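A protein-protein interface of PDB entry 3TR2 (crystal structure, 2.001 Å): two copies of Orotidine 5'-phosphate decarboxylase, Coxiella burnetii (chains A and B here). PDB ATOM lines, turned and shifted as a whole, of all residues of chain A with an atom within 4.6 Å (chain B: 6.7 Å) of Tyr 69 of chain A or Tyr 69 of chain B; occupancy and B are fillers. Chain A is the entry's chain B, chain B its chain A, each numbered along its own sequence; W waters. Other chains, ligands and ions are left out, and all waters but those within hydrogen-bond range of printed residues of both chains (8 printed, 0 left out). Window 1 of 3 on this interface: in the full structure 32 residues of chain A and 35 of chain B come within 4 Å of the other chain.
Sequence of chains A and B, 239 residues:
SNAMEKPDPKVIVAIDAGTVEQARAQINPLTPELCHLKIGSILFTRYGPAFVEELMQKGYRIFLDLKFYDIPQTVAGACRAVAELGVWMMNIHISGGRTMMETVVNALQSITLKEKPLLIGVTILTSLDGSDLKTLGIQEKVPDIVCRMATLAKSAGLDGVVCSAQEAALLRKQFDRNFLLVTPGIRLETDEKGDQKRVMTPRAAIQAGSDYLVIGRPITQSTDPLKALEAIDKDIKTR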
ATOM      1  N   LYS A  67      -8.235 -15.003  14.736  1.00  0.00           N
ATOM      2  CA  LYS A  67      -8.682 -15.295  13.373  1.00  0.00           C
ATOM      3  C   LYS A  67     -10.192 -15.088  13.176  1.00  0.00           C
ATOM      4  O   LYS A  67     -10.911 -16.029  12.826  1.00  0.00           O
ATOM      5  CB  LYS A  67      -8.293 -16.729  12.986  1.00  0.00           C
ATOM      6  CG  LYS A  67      -6.779 -17.022  12.987  1.00  0.00           C
ATOM      7  CD  LYS A  67      -6.502 -18.474  12.543  1.00  0.00           C
ATOM      8  CE  LYS A  67      -4.998 -18.796  12.500  1.00  0.00           C
ATOM      9  NZ  LYS A  67      -4.335 -18.748  13.845  1.00  0.00           N
ATOM     10  N   PHE A  68     -10.666 -13.863  13.389  1.00  0.00           N
ATOM     11  CA  PHE A  68     -12.089 -13.558  13.222  1.00  0.00           C
ATOM     12  C   PHE A  68     -12.553 -13.840  11.795  1.00  0.00           C
ATOM     13  O   PHE A  68     -11.831 -13.574  10.839  1.00  0.00           O
ATOM     14  CB  PHE A  68     -12.380 -12.093  13.554  1.00  0.00           C
ATOM     15  CG  PHE A  68     -12.085 -11.709  14.994  1.00  0.00           C
ATOM     16  CD1 PHE A  68     -12.770 -12.297  16.041  1.00  0.00           C
ATOM     17  CD2 PHE A  68     -11.135 -10.738  15.289  1.00  0.00           C
ATOM     18  CE1 PHE A  68     -12.492 -11.935  17.376  1.00  0.00           C
ATOM     19  CE2 PHE A  68     -10.863 -10.377  16.608  1.00  0.00           C
ATOM     20  CZ  PHE A  68     -11.543 -10.967  17.643  1.00  0.00           C
ATOM     21  N   TYR A  69     -13.767 -14.368  11.668  1.00  0.00           N
ATOM     22  CA  TYR A  69     -14.374 -14.653  10.371  1.00  0.00           C
ATOM     23  C   TYR A  69     -15.888 -14.695  10.620  1.00  0.00           C
ATOM     24  O   TYR A  69     -16.446 -15.716  11.029  1.00  0.00           O
ATOM     25  CB  TYR A  69     -13.834 -15.973   9.818  1.00  0.00           C
ATOM     26  CG  TYR A  69     -14.325 -16.397   8.438  1.00  0.00           C
ATOM     27  CD1 TYR A  69     -15.417 -15.790   7.835  1.00  0.00           C
ATOM     28  CD2 TYR A  69     -13.696 -17.434   7.751  1.00  0.00           C
ATOM     29  CE1 TYR A  69     -15.866 -16.199   6.578  1.00  0.00           C
ATOM     30  CE2 TYR A  69     -14.139 -17.852   6.501  1.00  0.00           C
ATOM     31  CZ  TYR A  69     -15.220 -17.229   5.919  1.00  0.00           C
ATOM     32  OH  TYR A  69     -15.667 -17.642   4.674  1.00  0.00           O
ATOM     33  N   ASP A  70     -16.523 -13.545  10.414  1.00  0.00           N
ATOM     34  CA  ASP A  70     -17.923 -13.331  10.751  1.00  0.00           C
ATOM     35  C   ASP A  70     -18.390 -12.150   9.905  1.00  0.00           C
ATOM     36  O   ASP A  70     -17.622 -11.636   9.082  1.00  0.00           O
ATOM     37  CB  ASP A  70     -18.062 -13.019  12.254  1.00  0.00           C
ATOM     38  CG  ASP A  70     -19.400 -13.468  12.832  1.00  0.00           C
ATOM     39  OD1 ASP A  70     -20.441 -13.286  12.167  1.00  0.00           O
ATOM     40  OD2 ASP A  70     -19.407 -14.008  13.959  1.00  0.00           O
ATOM     41  N   VAL A  75     -17.305  -8.514  13.242  1.00  0.00           N
ATOM     42  CA  VAL A  75     -15.844  -8.481  13.250  1.00  0.00           C
ATOM     43  C   VAL A  75     -15.315  -7.093  13.595  1.00  0.00           C
ATOM     44  O   VAL A  75     -14.342  -6.972  14.341  1.00  0.00           O
ATOM     45  CB  VAL A  75     -15.203  -8.943  11.922  1.00  0.00           C
ATOM     46  CG1 VAL A  75     -13.688  -8.974  12.074  1.00  0.00           C
ATOM     47  CG2 VAL A  75     -15.698 -10.320  11.535  1.00  0.00           C
ATOM     48  N   HIS A  93      -9.632 -13.451   8.985  1.00  0.00           N
ATOM     49  CA  HIS A  93      -9.628 -14.269   7.777  1.00  0.00           C
ATOM     50  C   HIS A  93      -9.973 -13.444   6.542  1.00  0.00           C
ATOM     51  O   HIS A  93     -11.028 -12.807   6.486  1.00  0.00           O
ATOM     52  CB  HIS A  93     -10.647 -15.400   7.907  1.00  0.00           C
ATOM     53  CG  HIS A  93     -10.094 -16.646   8.534  1.00  0.00           C
ATOM     54  ND1 HIS A  93      -9.360 -17.562   7.825  1.00  0.00           N
ATOM     55  CD2 HIS A  93     -10.194 -17.127   9.794  1.00  0.00           C
ATOM     56  CE1 HIS A  93      -9.016 -18.560   8.626  1.00  0.00           C
ATOM     57  NE2 HIS A  93      -9.511 -18.320   9.824  1.00  0.00           N
ATOM     58  N   SER A  95     -10.879 -14.663   3.894  1.00  0.00           N
ATOM     59  CA  SER A  95     -12.084 -15.336   3.397  1.00  0.00           C
ATOM     60  C   SER A  95     -13.362 -14.576   3.744  1.00  0.00           C
ATOM     61  O   SER A  95     -14.390 -14.736   3.077  1.00  0.00           O
ATOM     62  CB  SER A  95     -12.178 -16.754   3.967  1.00  0.00           C
ATOM     63  OG  SER A  95     -11.113 -17.571   3.520  1.00  0.00           O
ATOM     64  N   GLY A  96     -13.306 -13.774   4.811  1.00  0.00           N
ATOM     65  CA  GLY A  96     -14.446 -12.978   5.232  1.00  0.00           C
ATOM     66  C   GLY A  96     -14.935 -11.994   4.185  1.00  0.00           C
ATOM     67  O   GLY A  96     -16.076 -11.551   4.251  1.00  0.00           O
ATOM     68  N   MET A 100     -16.202  -6.896   4.853  1.00  0.00           N
ATOM     69  CA  MET A 100     -15.779  -7.145   6.231  1.00  0.00           C
ATOM     70  C   MET A 100     -14.456  -6.450   6.544  1.00  0.00           C
ATOM     71  O   MET A 100     -14.339  -5.729   7.540  1.00  0.00           O
ATOM     72  CB  MET A 100     -15.625  -8.639   6.486  1.00  0.00           C
ATOM     73  CG  MET A 100     -15.272  -8.970   7.938  1.00  0.00           C
ATOM     74  SD  MET A 100     -14.478 -10.737   8.094  1.00  0.00           S
ATOM     75  CE  MET A 100     -12.796 -10.319   7.189  1.00  0.00           C
ATOM     76  N   LEU A 125      -5.015 -21.644   5.707  1.00  0.00           N
ATOM     77  CA  LEU A 125      -4.316 -22.342   6.784  1.00  0.00           C
ATOM     78  C   LEU A 125      -3.574 -23.548   6.228  1.00  0.00           C
ATOM     79  O   LEU A 125      -4.056 -24.207   5.309  1.00  0.00           O
ATOM     80  CB  LEU A 125      -5.287 -22.806   7.866  1.00  0.00           C
ATOM     81  CG  LEU A 125      -6.037 -21.736   8.662  1.00  0.00           C
ATOM     82  CD1 LEU A 125      -6.921 -22.391   9.709  1.00  0.00           C
ATOM     83  CD2 LEU A 125      -5.061 -20.764   9.311  1.00  0.00           C
ATOM     84  N   LEU A 128      -5.379 -26.960   5.683  1.00  0.00           N
ATOM     85  CA  LEU A 128      -6.255 -27.293   4.564  1.00  0.00           C
ATOM     86  C   LEU A 128      -5.467 -28.024   3.487  1.00  0.00           C
ATOM     87  O   LEU A 128      -4.456 -27.515   2.994  1.00  0.00           O
ATOM     88  CB  LEU A 128      -6.888 -26.039   3.967  1.00  0.00           C
ATOM     89  CG  LEU A 128      -8.267 -25.658   4.504  1.00  0.00           C
ATOM     90  CD1 LEU A 128      -8.172 -25.233   5.948  1.00  0.00           C
ATOM     91  CD2 LEU A 128      -8.881 -24.555   3.657  1.00  0.00           C
ATOM     92  N   LEU B  66     -18.737 -18.037  18.304  1.00  0.00           N
ATOM     93  CA  LEU B  66     -17.383 -17.513  18.049  1.00  0.00           C
ATOM     94  C   LEU B  66     -16.799 -17.937  16.688  1.00  0.00           C
ATOM     95  O   LEU B  66     -15.736 -17.460  16.275  1.00  0.00           O
ATOM     96  CB  LEU B  66     -16.434 -17.928  19.179  1.00  0.00           C
ATOM     97  CG  LEU B  66     -16.934 -17.606  20.591  1.00  0.00           C
ATOM     98  CD1 LEU B  66     -15.881 -17.977  21.665  1.00  0.00           C
ATOM     99  CD2 LEU B  66     -17.323 -16.123  20.705  1.00  0.00           C
ATOM    100  N   LYS B  67     -17.497 -18.825  15.994  1.00  0.00           N
ATOM    101  CA  LYS B  67     -17.100 -19.239  14.642  1.00  0.00           C
ATOM    102  C   LYS B  67     -15.607 -19.543  14.531  1.00  0.00           C
ATOM    103  O   LYS B  67     -14.883 -18.885  13.772  1.00  0.00           O
ATOM    104  CB  LYS B  67     -17.506 -18.181  13.607  1.00  0.00           C
ATOM    105  CG  LYS B  67     -19.001 -17.847  13.608  1.00  0.00           C
ATOM    106  CD  LYS B  67     -19.435 -17.082  12.362  1.00  0.00           C
ATOM    107  CE  LYS B  67     -20.951 -16.893  12.346  1.00  0.00           C
ATOM    108  NZ  LYS B  67     -21.472 -16.081  13.486  1.00  0.00           N
ATOM    109  N   PHE B  68     -15.145 -20.542  15.283  1.00  0.00           N
ATOM    110  CA  PHE B  68     -13.732 -20.911  15.250  1.00  0.00           C
ATOM    111  C   PHE B  68     -13.319 -21.394  13.865  1.00  0.00           C
ATOM    112  O   PHE B  68     -14.040 -22.161  13.224  1.00  0.00           O
ATOM    113  CB  PHE B  68     -13.437 -22.018  16.260  1.00  0.00           C
ATOM    114  CG  PHE B  68     -13.658 -21.616  17.686  1.00  0.00           C
ATOM    115  CD1 PHE B  68     -12.858 -20.651  18.279  1.00  0.00           C
ATOM    116  CD2 PHE B  68     -14.639 -22.223  18.443  1.00  0.00           C
ATOM    117  CE1 PHE B  68     -13.044 -20.287  19.602  1.00  0.00           C
ATOM    118  CE2 PHE B  68     -14.827 -21.860  19.763  1.00  0.00           C
ATOM    119  CZ  PHE B  68     -14.025 -20.891  20.341  1.00  0.00           C
ATOM    120  N   TYR B  69     -12.159 -20.934  13.413  1.00  0.00           N
ATOM    121  CA  TYR B  69     -11.575 -21.375  12.150  1.00  0.00           C
ATOM    122  C   TYR B  69     -10.058 -21.289  12.322  1.00  0.00           C
ATOM    123  O   TYR B  69      -9.442 -20.248  12.099  1.00  0.00           O
ATOM    124  CB  TYR B  69     -12.080 -20.492  11.007  1.00  0.00           C
ATOM    125  CG  TYR B  69     -11.612 -20.853   9.607  1.00  0.00           C
ATOM    126  CD1 TYR B  69     -10.514 -21.678   9.393  1.00  0.00           C
ATOM    127  CD2 TYR B  69     -12.265 -20.335   8.492  1.00  0.00           C
ATOM    128  CE1 TYR B  69     -10.081 -21.983   8.096  1.00  0.00           C
ATOM    129  CE2 TYR B  69     -11.845 -20.628   7.208  1.00  0.00           C
ATOM    130  CZ  TYR B  69     -10.757 -21.452   7.011  1.00  0.00           C
ATOM    131  OH  TYR B  69     -10.343 -21.736   5.729  1.00  0.00           O
ATOM    132  N   ASP B  70      -9.467 -22.390  12.757  1.00  0.00           N
ATOM    133  CA  ASP B  70      -8.048 -22.403  13.067  1.00  0.00           C
ATOM    134  C   ASP B  70      -7.535 -23.817  12.805  1.00  0.00           C
ATOM    135  O   ASP B  70      -8.281 -24.664  12.311  1.00  0.00           O
ATOM    136  CB  ASP B  70      -7.838 -21.986  14.528  1.00  0.00           C
ATOM    137  CG  ASP B  70      -6.493 -21.308  14.757  1.00  0.00           C
ATOM    138  OD1 ASP B  70      -5.464 -21.813  14.256  1.00  0.00           O
ATOM    139  OD2 ASP B  70      -6.472 -20.266  15.432  1.00  0.00           O
ATOM    140  N   ILE B  71      -6.269 -24.086  13.110  1.00  0.00           N
ATOM    141  CA  ILE B  71      -5.760 -25.440  12.930  1.00  0.00           C
ATOM    142  C   ILE B  71      -6.433 -26.389  13.926  1.00  0.00           C
ATOM    143  O   ILE B  71      -6.878 -25.958  14.997  1.00  0.00           O
ATOM    144  CB  ILE B  71      -4.215 -25.513  13.023  1.00  0.00           C
ATOM    145  CG1 ILE B  71      -3.731 -25.232  14.447  1.00  0.00           C
ATOM    146  CG2 ILE B  71      -3.579 -24.543  12.033  1.00  0.00           C
ATOM    147  CD1 ILE B  71      -2.216 -25.196  14.574  1.00  0.00           C
ATOM    148  N   VAL B  75      -8.443 -25.401  17.509  1.00  0.00           N
ATOM    149  CA  VAL B  75      -9.897 -25.412  17.633  1.00  0.00           C
ATOM    150  C   VAL B  75     -10.343 -26.472  18.644  1.00  0.00           C
ATOM    151  O   VAL B  75     -11.263 -26.242  19.425  1.00  0.00           O
ATOM    152  CB  VAL B  75     -10.608 -25.617  16.278  1.00  0.00           C
ATOM    153  CG1 VAL B  75     -12.119 -25.463  16.451  1.00  0.00           C
ATOM    154  CG2 VAL B  75     -10.100 -24.611  15.257  1.00  0.00           C
ATOM    155  N   ASN B  91     -20.173 -23.116  17.629  1.00  0.00           N
ATOM    156  CA  ASN B  91     -20.026 -23.313  16.194  1.00  0.00           C
ATOM    157  C   ASN B  91     -18.608 -23.162  15.659  1.00  0.00           C
ATOM    158  O   ASN B  91     -17.742 -22.524  16.272  1.00  0.00           O
ATOM    159  CB  ASN B  91     -21.026 -22.458  15.389  1.00  0.00           C
ATOM    160  CG  ASN B  91     -20.846 -20.960  15.601  1.00  0.00           C
ATOM    161  OD1 ASN B  91     -19.964 -20.506  16.342  1.00  0.00           O
ATOM    162  ND2 ASN B  91     -21.691 -20.180  14.934  1.00  0.00           N
ATOM    163  N   ILE B  92     -18.375 -23.778  14.506  1.00  0.00           N
ATOM    164  CA  ILE B  92     -17.067 -23.740  13.869  1.00  0.00           C
ATOM    165  C   ILE B  92     -17.240 -23.640  12.363  1.00  0.00           C
ATOM    166  O   ILE B  92     -18.247 -24.094  11.826  1.00  0.00           O
ATOM    167  CB  ILE B  92     -16.262 -25.004  14.192  1.00  0.00           C
ATOM    168  CG1 ILE B  92     -16.976 -26.235  13.625  1.00  0.00           C
ATOM    169  CG2 ILE B  92     -16.067 -25.131  15.702  1.00  0.00           C
ATOM    170  CD1 ILE B  92     -16.349 -27.555  14.057  1.00  0.00           C
ATOM    171  N   HIS B  93     -16.257 -23.043  11.693  1.00  0.00           N
ATOM    172  CA  HIS B  93     -16.281 -22.922  10.239  1.00  0.00           C
ATOM    173  C   HIS B  93     -15.991 -24.255   9.571  1.00  0.00           C
ATOM    174  O   HIS B  93     -14.926 -24.843   9.762  1.00  0.00           O
ATOM    175  CB  HIS B  93     -15.258 -21.889   9.758  1.00  0.00           C
ATOM    176  CG  HIS B  93     -15.804 -20.502   9.658  1.00  0.00           C
ATOM    177  ND1 HIS B  93     -16.540 -20.070   8.570  1.00  0.00           N
ATOM    178  CD2 HIS B  93     -15.723 -19.447  10.498  1.00  0.00           C
ATOM    179  CE1 HIS B  93     -16.887 -18.813   8.753  1.00  0.00           C
ATOM    180  NE2 HIS B  93     -16.405 -18.406   9.914  1.00  0.00           N
ATOM    181  N   ILE B  94     -16.941 -24.724   8.772  1.00  0.00           N
ATOM    182  CA  ILE B  94     -16.749 -25.939   7.989  1.00  0.00           C
ATOM    183  C   ILE B  94     -15.583 -25.764   7.009  1.00  0.00           C
ATOM    184  O   ILE B  94     -14.907 -26.732   6.660  1.00  0.00           O
ATOM    185  CB  ILE B  94     -18.050 -26.327   7.253  1.00  0.00           C
ATOM    186  CG1 ILE B  94     -19.129 -26.685   8.276  1.00  0.00           C
ATOM    187  CG2 ILE B  94     -17.807 -27.497   6.293  1.00  0.00           C
ATOM    188  CD1 ILE B  94     -20.558 -26.639   7.745  1.00  0.00           C
ATOM    189  N   SER B  95     -15.348 -24.528   6.579  1.00  0.00           N
ATOM    190  CA  SER B  95     -14.199 -24.209   5.721  1.00  0.00           C
ATOM    191  C   SER B  95     -12.877 -24.726   6.302  1.00  0.00           C
ATOM    192  O   SER B  95     -11.911 -24.944   5.576  1.00  0.00           O
ATOM    193  CB  SER B  95     -14.078 -22.695   5.538  1.00  0.00           C
ATOM    194  OG  SER B  95     -15.129 -22.184   4.745  1.00  0.00           O
ATOM    195  N   GLY B  96     -12.840 -24.905   7.618  1.00  0.00           N
ATOM    196  CA  GLY B  96     -11.627 -25.311   8.310  1.00  0.00           C
ATOM    197  C   GLY B  96     -11.108 -26.687   7.935  1.00  0.00           C
ATOM    198  O   GLY B  96      -9.978 -27.034   8.274  1.00  0.00           O
ATOM    199  N   GLY B  97     -11.926 -27.483   7.252  1.00  0.00           N
ATOM    200  CA  GLY B  97     -11.471 -28.766   6.742  1.00  0.00           C
ATOM    201  C   GLY B  97     -11.958 -29.976   7.522  1.00  0.00           C
ATOM    202  O   GLY B  97     -12.408 -29.866   8.664  1.00  0.00           O
ATOM    203  N   MET B 100      -9.825 -30.836  10.876  1.00  0.00           N
ATOM    204  CA  MET B 100     -10.231 -29.946  11.957  1.00  0.00           C
ATOM    205  C   MET B 100     -11.545 -30.400  12.584  1.00  0.00           C
ATOM    206  O   MET B 100     -11.634 -30.578  13.801  1.00  0.00           O
ATOM    207  CB  MET B 100     -10.371 -28.514  11.451  1.00  0.00           C
ATOM    208  CG  MET B 100     -10.545 -27.495  12.574  1.00  0.00           C
ATOM    209  SD  MET B 100     -11.460 -25.893  11.960  1.00  0.00           S
ATOM    210  CE  MET B 100     -13.126 -26.738  11.418  1.00  0.00           C
ATOM    211  N   VAL B 122     -20.705 -23.763  10.500  1.00  0.00           N
ATOM    212  CA  VAL B 122     -20.995 -22.574   9.717  1.00  0.00           C
ATOM    213  C   VAL B 122     -20.592 -22.858   8.277  1.00  0.00           C
ATOM    214  O   VAL B 122     -19.487 -23.330   8.039  1.00  0.00           O
ATOM    215  CB  VAL B 122     -20.176 -21.369  10.232  1.00  0.00           C
ATOM    216  CG1 VAL B 122     -20.357 -20.177   9.325  1.00  0.00           C
ATOM    217  CG2 VAL B 122     -20.554 -21.028  11.691  1.00  0.00           C
ATOM    218  N   THR B 123     -21.479 -22.590   7.321  1.00  0.00           N
ATOM    219  CA  THR B 123     -21.162 -22.837   5.920  1.00  0.00           C
ATOM    220  C   THR B 123     -20.529 -21.597   5.287  1.00  0.00           C
ATOM    221  O   THR B 123     -19.388 -21.255   5.586  1.00  0.00           O
ATOM    222  CB  THR B 123     -22.405 -23.279   5.109  1.00  0.00           C
ATOM    223  OG1 THR B 123     -23.401 -22.250   5.149  1.00  0.00           O
ATOM    224  CG2 THR B 123     -22.983 -24.562   5.687  1.00  0.00           C
ATOM    225  N   ILE B 124     -21.273 -20.939   4.411  1.00  0.00           N
ATOM    226  CA  ILE B 124     -20.842 -19.693   3.791  1.00  0.00           C
ATOM    227  C   ILE B 124     -21.677 -18.574   4.392  1.00  0.00           C
ATOM    228  O   ILE B 124     -22.897 -18.593   4.275  1.00  0.00           O
ATOM    229  CB  ILE B 124     -21.089 -19.717   2.263  1.00  0.00           C
ATOM    230  CG1 ILE B 124     -20.277 -20.838   1.586  1.00  0.00           C
ATOM    231  CG2 ILE B 124     -20.821 -18.349   1.648  1.00  0.00           C
ATOM    232  CD1 ILE B 124     -18.759 -20.648   1.627  1.00  0.00           C
ATOM    233  N   LEU B 125     -21.037 -17.600   5.041  1.00  0.00           N
ATOM    234  CA  LEU B 125     -21.778 -16.512   5.689  1.00  0.00           C
ATOM    235  C   LEU B 125     -22.790 -15.879   4.746  1.00  0.00           C
ATOM    236  O   LEU B 125     -22.563 -15.854   3.536  1.00  0.00           O
ATOM    237  CB  LEU B 125     -20.824 -15.417   6.169  1.00  0.00           C
ATOM    238  CG  LEU B 125     -19.723 -15.785   7.160  1.00  0.00           C
ATOM    239  CD1 LEU B 125     -18.870 -14.545   7.437  1.00  0.00           C
ATOM    240  CD2 LEU B 125     -20.307 -16.360   8.452  1.00  0.00           C
ATOM    241  N   SER B 127     -23.187 -12.843   4.621  1.00  0.00           N
ATOM    242  CA  SER B 127     -22.522 -11.617   4.191  1.00  0.00           C
ATOM    243  C   SER B 127     -21.692 -11.810   2.916  1.00  0.00           C
ATOM    244  O   SER B 127     -21.198 -10.844   2.332  1.00  0.00           O
ATOM    245  CB  SER B 127     -21.649 -11.059   5.317  1.00  0.00           C
ATOM    246  OG  SER B 127     -20.673 -12.003   5.711  1.00  0.00           O
ATOM    247  N   LEU B 128     -21.524 -13.061   2.495  1.00  0.00           N
ATOM    248  CA  LEU B 128     -20.775 -13.368   1.281  1.00  0.00           C
ATOM    249  C   LEU B 128     -21.690 -13.918   0.193  1.00  0.00           C
ATOM    250  O   LEU B 128     -22.650 -14.633   0.489  1.00  0.00           O
ATOM    251  CB  LEU B 128     -19.683 -14.398   1.574  1.00  0.00           C
ATOM    252  CG  LEU B 128     -18.621 -14.012   2.607  1.00  0.00           C
ATOM    253  CD1 LEU B 128     -17.971 -15.263   3.172  1.00  0.00           C
ATOM    254  CD2 LEU B 128     -17.577 -13.070   2.000  1.00  0.00           C
HETATM  255  O   HOH W   1     -14.651 -15.793  14.082  1.00  0.00           O
HETATM  256  O   HOH W   2     -18.289 -11.390   6.237  1.00  0.00           O
HETATM  257  O   HOH W   3     -11.598 -20.215   3.896  1.00  0.00           O
HETATM  258  O   HOH W   4      -7.668 -20.496   5.885  1.00  0.00           O
HETATM  259  O   HOH W   5     -14.552 -19.906   3.648  1.00  0.00           O
HETATM  260  O   HOH W   6     -18.417 -18.423   5.529  1.00  0.00           O
HETATM  261  O   HOH W   7     -16.959 -14.587  15.164  1.00  0.00           O
HETATM  262  O   HOH W   8     -11.143 -18.523  14.786  1.00  0.00           O
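O of Tyr 69 of chain B touches CD of Lys 67 of chain A, at 3.5 Å. Lys 67 of chain B touches Tyr 69 of chain A. Tyr 69 of chain B touches Tyr 69 of chain A. Tyr 69 of chain A touches Leu 125 of chain B (CE1 to CD1, 3.5 Å). Leu 128 of chain B touches Tyr 69 of chain A. Leu 125 of chain A touches Tyr 69 of chain B. CD1 of Leu 125 of chain A touches N of Ile 71 of chain B (3.9 Å). Leu 128 of chain A touches Tyr 69 of chain B (CD2 to OH, 3.8 Å). CD2 of Leu 128 of chain A touches O of Ser 95 of chain B, at 3.6 Å. Leu 128 of chain A touches Gly 96 of chain B.
The side-chain amide oxygen (OD1) of Asn 91 of chain B is in hydrogen-bond range of the backbone NH (N) of Lys 67 of chain B (3.0 Å). N of His 93 of chain B is in hydrogen-bond range of O of Phe 68 of chain B, 2.8 Å away. O of Phe 68 of chain A is in hydrogen-bond range of N of His 93 of chain A, at 2.9 Å.
NZ of Lys 67 of chain B lies within salt-bridge range of OD2 of Asp 70 of chain A (3.0 Å). The backbone carbonyl oxygen (O) of Tyr 69 of chain B sits at hydrogen-bond distance from a ring nitrogen (NE2) of His 93 of chain A, 3.0 Å away. The side-chain amino group (NZ) of Lys 67 of chain A is in salt-bridge range of the side-chain carboxylate (OD2) of Asp 70 of chain B, 3.1 Å away. The backbone carbonyl oxygen of Tyr 69 of chain A lies within hydrogen-bond range of a ring nitrogen (NE2) of His 93 of chain B, at 2.9 Å.
Lys 67 of chain A touches Tyr 69 of chain B, and with the chains exchanged Tyr 69 of chain A touches Lys 67 of chain B. Lys 67 of chain A touches Asp 70 of chain B, and with the chains exchanged Asp 70 of chain A touches Lys 67 of chain B. Tyr 69 of chain A touches its own counterpart, Tyr 69 of chain B. Ser 95 of chain A touches Leu 128 of chain B, and with the chains exchanged Leu 128 of chain A touches Ser 95 of chain B. Of the 18 pairs that touch across the chains among the printed residues, 17 have their exchanged pair printed and touching as well.
Of the 21 printed residues of chain B, 9 touch a printed residue of chain A. Hydrophobic or aromatic side chains of chain A within 4 Å of the printed part of chain B: Tyr 69, His 93, Leu 125 and Leu 128. Among the printed residues, 18 pairs touch across the chains. Among the printed residues, Asp or Glu carboxylates within 4 Å of a Lys or Arg side-chain nitrogen of the other chain: Lys 67 of chain A with Asp 70 of chain B and Asp 70 of chain A with Lys 67 of chain B.
Phe 68 of chain A touches none of the printed residues of chain B. Tyr 69 of chain A touches just these residues of chain B: Lys 67, Tyr 69, His 93, Leu 125 and Leu 128. Of the printed residues of chain B, Asp 70 of chain A touches Lys 67 (3.0 Å) and Leu 125 (3.5 Å). Tyr 69 of chain B touches five residues of chain A. Printed residues of chain A within 4 Å of Ile 71 of chain B: Leu 125 (3.9 Å). Of the printed residues of chain A, Leu 125 of chain B touches Tyr 69 (3.5 Å) and Asp 70 (3.5 Å). The nearest printed residue of chain A that does not touch Tyr 69 of chain B is Ser 95 of chain A (4.8 Å). The nearest printed residue of chain A that does not touch Lys 67 of chain B is Lys 67 of chain A (5.0 Å).
Water W2 lies within hydrogen-bond range of the side-chain hydroxyl of Ser 127 of chain B, the backbone carbonyl oxygen of Asp 70 of chain A and the backbone carbonyl oxygen of Gly 96 of chain A. Water W5 lies within hydrogen-bond range of the side-chain hydroxyl (OG) of Ser 95 of chain B (2.6 Å) and the side-chain hydroxyl (OH) of Tyr 69 of chain A (2.7 Å). Water W3 lies within hydrogen-bond range of the side-chain hydroxyl of Tyr 69 of chain B (2.7 Å) and the side-chain hydroxyl of Ser 95 of chain A (2.7 Å). Water W7 bridges the side-chain carboxylate of Asp 70 of chain A and the backbone carbonyl oxygen of Leu 66 of chain B. Water W6 lies within hydrogen-bond range of N of Leu 125 of chain B (2.8 Å), OH of Tyr 69 of chain A (3.0 Å) and O of Thr 123 of chain B (3.0 Å). Water W1 lies within hydrogen-bond range of N of Tyr 69 of chain A (2.9 Å), O of Leu 66 of chain B (3.0 Å) and O of Lys 67 of chain B (3.1 Å).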
